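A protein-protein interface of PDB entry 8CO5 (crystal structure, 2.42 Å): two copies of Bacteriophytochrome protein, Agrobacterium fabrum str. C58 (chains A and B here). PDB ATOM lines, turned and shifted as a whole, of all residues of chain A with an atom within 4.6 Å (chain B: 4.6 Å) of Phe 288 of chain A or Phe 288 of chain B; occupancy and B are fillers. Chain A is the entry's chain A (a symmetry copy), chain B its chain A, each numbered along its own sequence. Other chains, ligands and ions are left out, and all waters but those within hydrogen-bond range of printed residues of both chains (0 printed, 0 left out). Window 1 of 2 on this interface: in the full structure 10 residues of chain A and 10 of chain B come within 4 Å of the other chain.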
ATOM      1  N   ALA A 125     -25.663  -4.886 -24.341  1.00  0.00           N
ATOM      2  CA  ALA A 125     -24.795  -5.924 -23.735  1.00  0.00           C
ATOM      3  C   ALA A 125     -24.772  -7.167 -24.633  1.00  0.00           C
ATOM      4  O   ALA A 125     -23.699  -7.795 -24.749  1.00  0.00           O
ATOM      5  CB  ALA A 125     -25.278  -6.257 -22.346  1.00  0.00           C
ATOM      6  N   GLU A 284     -27.017   5.511 -12.800  1.00  0.00           N
ATOM      7  CA  GLU A 284     -26.304   4.234 -12.522  1.00  0.00           C
ATOM      8  C   GLU A 284     -26.404   3.317 -13.748  1.00  0.00           C
ATOM      9  O   GLU A 284     -25.474   2.515 -13.957  1.00  0.00           O
ATOM     10  CB  GLU A 284     -26.870   3.561 -11.270  1.00  0.00           C
ATOM     11  CG  GLU A 284     -26.192   4.016  -9.988  1.00  0.00           C
ATOM     12  CD  GLU A 284     -26.883   3.584  -8.705  1.00  0.00           C
ATOM     13  OE1 GLU A 284     -27.774   2.714  -8.776  1.00  0.00           O
ATOM     14  OE2 GLU A 284     -26.529   4.121  -7.637  1.00  0.00           O
ATOM     15  N   ALA A 285     -27.489   3.437 -14.520  1.00  0.00           N
ATOM     16  CA  ALA A 285     -27.727   2.684 -15.775  1.00  0.00           C
ATOM     17  C   ALA A 285     -26.763   3.173 -16.864  1.00  0.00           C
ATOM     18  O   ALA A 285     -26.375   2.352 -17.719  1.00  0.00           O
ATOM     19  CB  ALA A 285     -29.168   2.828 -16.204  1.00  0.00           C
ATOM     20  N   CYS A 286     -26.398   4.459 -16.827  1.00  0.00           N
ATOM     21  CA  CYS A 286     -25.466   5.116 -17.785  1.00  0.00           C
ATOM     22  C   CYS A 286     -24.013   4.800 -17.405  1.00  0.00           C
ATOM     23  O   CYS A 286     -23.212   4.525 -18.323  1.00  0.00           O
ATOM     24  CB  CYS A 286     -25.686   6.623 -17.820  1.00  0.00           C
ATOM     25  SG  CYS A 286     -27.341   7.097 -18.388  1.00  0.00           S
ATOM     26  N   ASP A 287     -23.691   4.845 -16.107  1.00  0.00           N
ATOM     27  CA  ASP A 287     -22.374   4.447 -15.539  1.00  0.00           C
ATOM     28  C   ASP A 287     -22.087   2.990 -15.919  1.00  0.00           C
ATOM     29  O   ASP A 287     -20.901   2.629 -16.053  1.00  0.00           O
ATOM     30  CB  ASP A 287     -22.349   4.632 -14.019  1.00  0.00           C
ATOM     31  CG  ASP A 287     -21.053   4.191 -13.357  1.00  0.00           C
ATOM     32  OD1 ASP A 287     -19.997   4.279 -14.013  1.00  0.00           O
ATOM     33  OD2 ASP A 287     -21.112   3.762 -12.187  1.00  0.00           O
ATOM     34  N   PHE A 288     -23.150   2.204 -16.095  1.00  0.00           N
ATOM     35  CA  PHE A 288     -23.123   0.734 -16.316  1.00  0.00           C
ATOM     36  C   PHE A 288     -22.908   0.439 -17.806  1.00  0.00           C
ATOM     37  O   PHE A 288     -22.178  -0.521 -18.123  1.00  0.00           O
ATOM     38  CB  PHE A 288     -24.415   0.129 -15.763  1.00  0.00           C
ATOM     39  CG  PHE A 288     -24.579  -1.355 -15.962  1.00  0.00           C
ATOM     40  CD1 PHE A 288     -23.942  -2.259 -15.126  1.00  0.00           C
ATOM     41  CD2 PHE A 288     -25.395  -1.847 -16.967  1.00  0.00           C
ATOM     42  CE1 PHE A 288     -24.104  -3.624 -15.305  1.00  0.00           C
ATOM     43  CE2 PHE A 288     -25.557  -3.212 -17.144  1.00  0.00           C
ATOM     44  CZ  PHE A 288     -24.912  -4.098 -16.313  1.00  0.00           C
ATOM     45  N   ALA A 289     -23.519   1.241 -18.686  1.00  0.00           N
ATOM     46  CA  ALA A 289     -23.330   1.196 -20.156  1.00  0.00           C
ATOM     47  C   ALA A 289     -21.894   1.609 -20.493  1.00  0.00           C
ATOM     48  O   ALA A 289     -21.309   1.022 -21.426  1.00  0.00           O
ATOM     49  CB  ALA A 289     -24.334   2.095 -20.838  1.00  0.00           C
ATOM     50  N   ALA A 290     -21.356   2.584 -19.754  1.00  0.00           N
ATOM     51  CA  ALA A 290     -19.973   3.100 -19.889  1.00  0.00           C
ATOM     52  C   ALA A 290     -18.972   1.992 -19.540  1.00  0.00           C
ATOM     53  O   ALA A 290     -17.893   1.955 -20.162  1.00  0.00           O
ATOM     54  CB  ALA A 290     -19.781   4.308 -19.007  1.00  0.00           C
ATOM     55  N   GLN A 291     -19.324   1.129 -18.582  1.00  0.00           N
ATOM     56  CA  GLN A 291     -18.486  -0.018 -18.139  1.00  0.00           C
ATOM     57  C   GLN A 291     -18.548  -1.131 -19.194  1.00  0.00           C
ATOM     58  O   GLN A 291     -17.497  -1.744 -19.454  1.00  0.00           O
ATOM     59  CB  GLN A 291     -18.917  -0.502 -16.752  1.00  0.00           C
ATOM     60  CG  GLN A 291     -18.262   0.278 -15.618  1.00  0.00           C
ATOM     61  CD  GLN A 291     -18.717  -0.153 -14.244  1.00  0.00           C
ATOM     62  OE1 GLN A 291     -19.034   0.673 -13.391  1.00  0.00           O
ATOM     63  NE2 GLN A 291     -18.749  -1.455 -14.011  1.00  0.00           N
ATOM     64  N   LEU A 292     -19.725  -1.369 -19.787  1.00  0.00           N
ATOM     65  CA  LEU A 292     -19.916  -2.350 -20.891  1.00  0.00           C
ATOM     66  C   LEU A 292     -19.026  -1.949 -22.073  1.00  0.00           C
ATOM     67  O   LEU A 292     -18.262  -2.808 -22.556  1.00  0.00           O
ATOM     68  CB  LEU A 292     -21.391  -2.393 -21.308  1.00  0.00           C
ATOM     69  CG  LEU A 292     -22.362  -2.967 -20.277  1.00  0.00           C
ATOM     70  CD1 LEU A 292     -23.787  -2.947 -20.812  1.00  0.00           C
ATOM     71  CD2 LEU A 292     -21.967  -4.380 -19.871  1.00  0.00           C
ATOM     72  N   ALA B 125     -21.553  -6.968 -11.394  1.00  0.00           N
ATOM     73  CA  ALA B 125     -20.951  -6.200 -12.510  1.00  0.00           C
ATOM     74  C   ALA B 125     -19.998  -5.138 -11.951  1.00  0.00           C
ATOM     75  O   ALA B 125     -18.943  -4.901 -12.574  1.00  0.00           O
ATOM     76  CB  ALA B 125     -22.034  -5.579 -13.356  1.00  0.00           C
ATOM     77  N   GLU B 284     -32.797 -15.050 -18.564  1.00  0.00           N
ATOM     78  CA  GLU B 284     -32.034 -14.045 -19.354  1.00  0.00           C
ATOM     79  C   GLU B 284     -31.078 -13.285 -18.425  1.00  0.00           C
ATOM     80  O   GLU B 284     -30.016 -12.848 -18.908  1.00  0.00           O
ATOM     81  CB  GLU B 284     -32.987 -13.092 -20.080  1.00  0.00           C
ATOM     82  CG  GLU B 284     -33.406 -13.594 -21.451  1.00  0.00           C
ATOM     83  CD  GLU B 284     -34.547 -12.825 -22.099  1.00  0.00           C
ATOM     84  OE1 GLU B 284     -34.881 -11.731 -21.603  1.00  0.00           O
ATOM     85  OE2 GLU B 284     -35.100 -13.326 -23.098  1.00  0.00           O
ATOM     86  N   ALA B 285     -31.447 -13.137 -17.149  1.00  0.00           N
ATOM     87  CA  ALA B 285     -30.627 -12.490 -16.096  1.00  0.00           C
ATOM     88  C   ALA B 285     -29.422 -13.378 -15.759  1.00  0.00           C
ATOM     89  O   ALA B 285     -28.361 -12.824 -15.407  1.00  0.00           O
ATOM     90  CB  ALA B 285     -31.471 -12.216 -14.874  1.00  0.00           C
ATOM     91  N   CYS B 286     -29.586 -14.701 -15.866  1.00  0.00           N
ATOM     92  CA  CYS B 286     -28.536 -15.723 -15.596  1.00  0.00           C
ATOM     93  C   CYS B 286     -27.599 -15.846 -16.805  1.00  0.00           C
ATOM     94  O   CYS B 286     -26.373 -15.945 -16.590  1.00  0.00           O
ATOM     95  CB  CYS B 286     -29.156 -17.076 -15.269  1.00  0.00           C
ATOM     96  SG  CYS B 286     -30.178 -17.057 -13.772  1.00  0.00           S
ATOM     97  N   ASP B 287     -28.159 -15.848 -18.020  1.00  0.00           N
ATOM     98  CA  ASP B 287     -27.408 -15.831 -19.306  1.00  0.00           C
ATOM     99  C   ASP B 287     -26.505 -14.592 -19.339  1.00  0.00           C
ATOM    100  O   ASP B 287     -25.440 -14.644 -19.986  1.00  0.00           O
ATOM    101  CB  ASP B 287     -28.362 -15.844 -20.504  1.00  0.00           C
ATOM    102  CG  ASP B 287     -27.671 -15.768 -21.855  1.00  0.00           C
ATOM    103  OD1 ASP B 287     -26.530 -16.260 -21.962  1.00  0.00           O
ATOM    104  OD2 ASP B 287     -28.281 -15.216 -22.793  1.00  0.00           O
ATOM    105  N   PHE B 288     -26.928 -13.532 -18.647  1.00  0.00           N
ATOM    106  CA  PHE B 288     -26.308 -12.182 -18.651  1.00  0.00           C
ATOM    107  C   PHE B 288     -25.159 -12.137 -17.634  1.00  0.00           C
ATOM    108  O   PHE B 288     -24.129 -11.500 -17.928  1.00  0.00           O
ATOM    109  CB  PHE B 288     -27.394 -11.139 -18.379  1.00  0.00           C
ATOM    110  CG  PHE B 288     -26.921  -9.712 -18.287  1.00  0.00           C
ATOM    111  CD1 PHE B 288     -26.670  -8.971 -19.432  1.00  0.00           C
ATOM    112  CD2 PHE B 288     -26.758  -9.099 -17.055  1.00  0.00           C
ATOM    113  CE1 PHE B 288     -26.247  -7.654 -19.343  1.00  0.00           C
ATOM    114  CE2 PHE B 288     -26.336  -7.783 -16.968  1.00  0.00           C
ATOM    115  CZ  PHE B 288     -26.080  -7.062 -18.112  1.00  0.00           C
ATOM    116  N   ALA B 289     -25.334 -12.794 -16.482  1.00  0.00           N
ATOM    117  CA  ALA B 289     -24.298 -12.974 -15.436  1.00  0.00           C
ATOM    118  C   ALA B 289     -23.174 -13.859 -15.988  1.00  0.00           C
ATOM    119  O   ALA B 289     -21.998 -13.595 -15.666  1.00  0.00           O
ATOM    120  CB  ALA B 289     -24.909 -13.576 -14.194  1.00  0.00           C
ATOM    121  N   ALA B 290     -23.535 -14.867 -16.788  1.00  0.00           N
ATOM    122  CA  ALA B 290     -22.603 -15.808 -17.456  1.00  0.00           C
ATOM    123  C   ALA B 290     -21.727 -15.044 -18.456  1.00  0.00           C
ATOM    124  O   ALA B 290     -20.551 -15.422 -18.618  1.00  0.00           O
ATOM    125  CB  ALA B 290     -23.378 -16.909 -18.137  1.00  0.00           C
ATOM    126  N   GLN B 291     -22.286 -14.013 -19.098  1.00  0.00           N
ATOM    127  CA  GLN B 291     -21.573 -13.152 -20.080  1.00  0.00           C
ATOM    128  C   GLN B 291     -20.630 -12.201 -19.330  1.00  0.00           C
ATOM    129  O   GLN B 291     -19.509 -11.988 -19.825  1.00  0.00           O
ATOM    130  CB  GLN B 291     -22.569 -12.406 -20.972  1.00  0.00           C
ATOM    131  CG  GLN B 291     -23.020 -13.223 -22.176  1.00  0.00           C
ATOM    132  CD  GLN B 291     -24.042 -12.521 -23.038  1.00  0.00           C
ATOM    133  OE1 GLN B 291     -25.049 -13.103 -23.432  1.00  0.00           O
ATOM    134  NE2 GLN B 291     -23.791 -11.258 -23.347  1.00  0.00           N
ATOM    135  N   LEU B 292     -21.060 -11.668 -18.180  1.00  0.00           N
ATOM    136  CA  LEU B 292     -20.224 -10.805 -17.300  1.00  0.00           C
ATOM    137  C   LEU B 292     -18.989 -11.597 -16.855  1.00  0.00           C
ATOM    138  O   LEU B 292     -17.865 -11.085 -17.028  1.00  0.00           O
ATOM    139  CB  LEU B 292     -21.040 -10.341 -16.088  1.00  0.00           C
ATOM    140  CG  LEU B 292     -22.190  -9.377 -16.383  1.00  0.00           C
ATOM    141  CD1 LEU B 292     -22.917  -9.002 -15.101  1.00  0.00           C
ATOM    142  CD2 LEU B 292     -21.695  -8.128 -17.097  1.00  0.00           C
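Among the printed residues, merely in contact across the chains: Ala 125 of chain A with Phe 288 of chain B (3.5 Å), Ala 125 of chain A with Gln 291 of chain B (3.7 Å), Phe 288 of chain A with Ala 125 of chain B (3.5 Å), Phe 288 of chain A with Phe 288 of chain B (3.7 Å) and Gln 291 of chain A with Ala 125 of chain B (3.7 Å).
Of chain B, only Ala 125 (3.5 Å) and Phe 288 (3.7 Å) come within 4 Å of Phe 288 of chain A. Phe 288 of chain B touches just these residues of chain A: Ala 125 and Phe 288. Of the printed residues of chain A, Gln 291 of chain B touches Ala 125. Printed residues of chain B within 4 Å of Ala 125 of chain A: Phe 288 and Gln 291. The nearest printed residue of chain B that does not touch Phe 288 of chain A is Leu 292 of chain B (5.2 Å). The nearest printed residue of chain A that does not touch Phe 288 of chain B is Leu 292 of chain A (5.2 Å). The nearest printed residue of chain A that does not touch Gln 291 of chain B is Leu 292 of chain A (7.9 Å).
Ala 125 of chain A touches Phe 288 of chain B, and with the chains exchanged Phe 288 of chain A touches Ala 125 of chain B. Ala 125 of chain A touches Gln 291 of chain B, and with the chains exchanged Gln 291 of chain A touches Ala 125 of chain B. Phe 288 of chain B touches its own counterpart, Phe 288 of chain A. Of the 5 pairs that touch across the chains among the printed residues, 5 have their exchanged pair printed and touching as well.
Hydrophobic or aromatic side chains of chain B within 4 Å of the printed part of chain A: Ala 125 and Phe 288. Of the 10 printed residues of chain A, 3 touch a printed residue of chain B. Hydrophobic or aromatic side chains of chain A that line the printed part of chain B: Ala 125 and Phe 288. Among the printed residues, no Asp or Glu carboxylate lies within 4 Å of a Lys or Arg side-chain nitrogen of the other chain.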
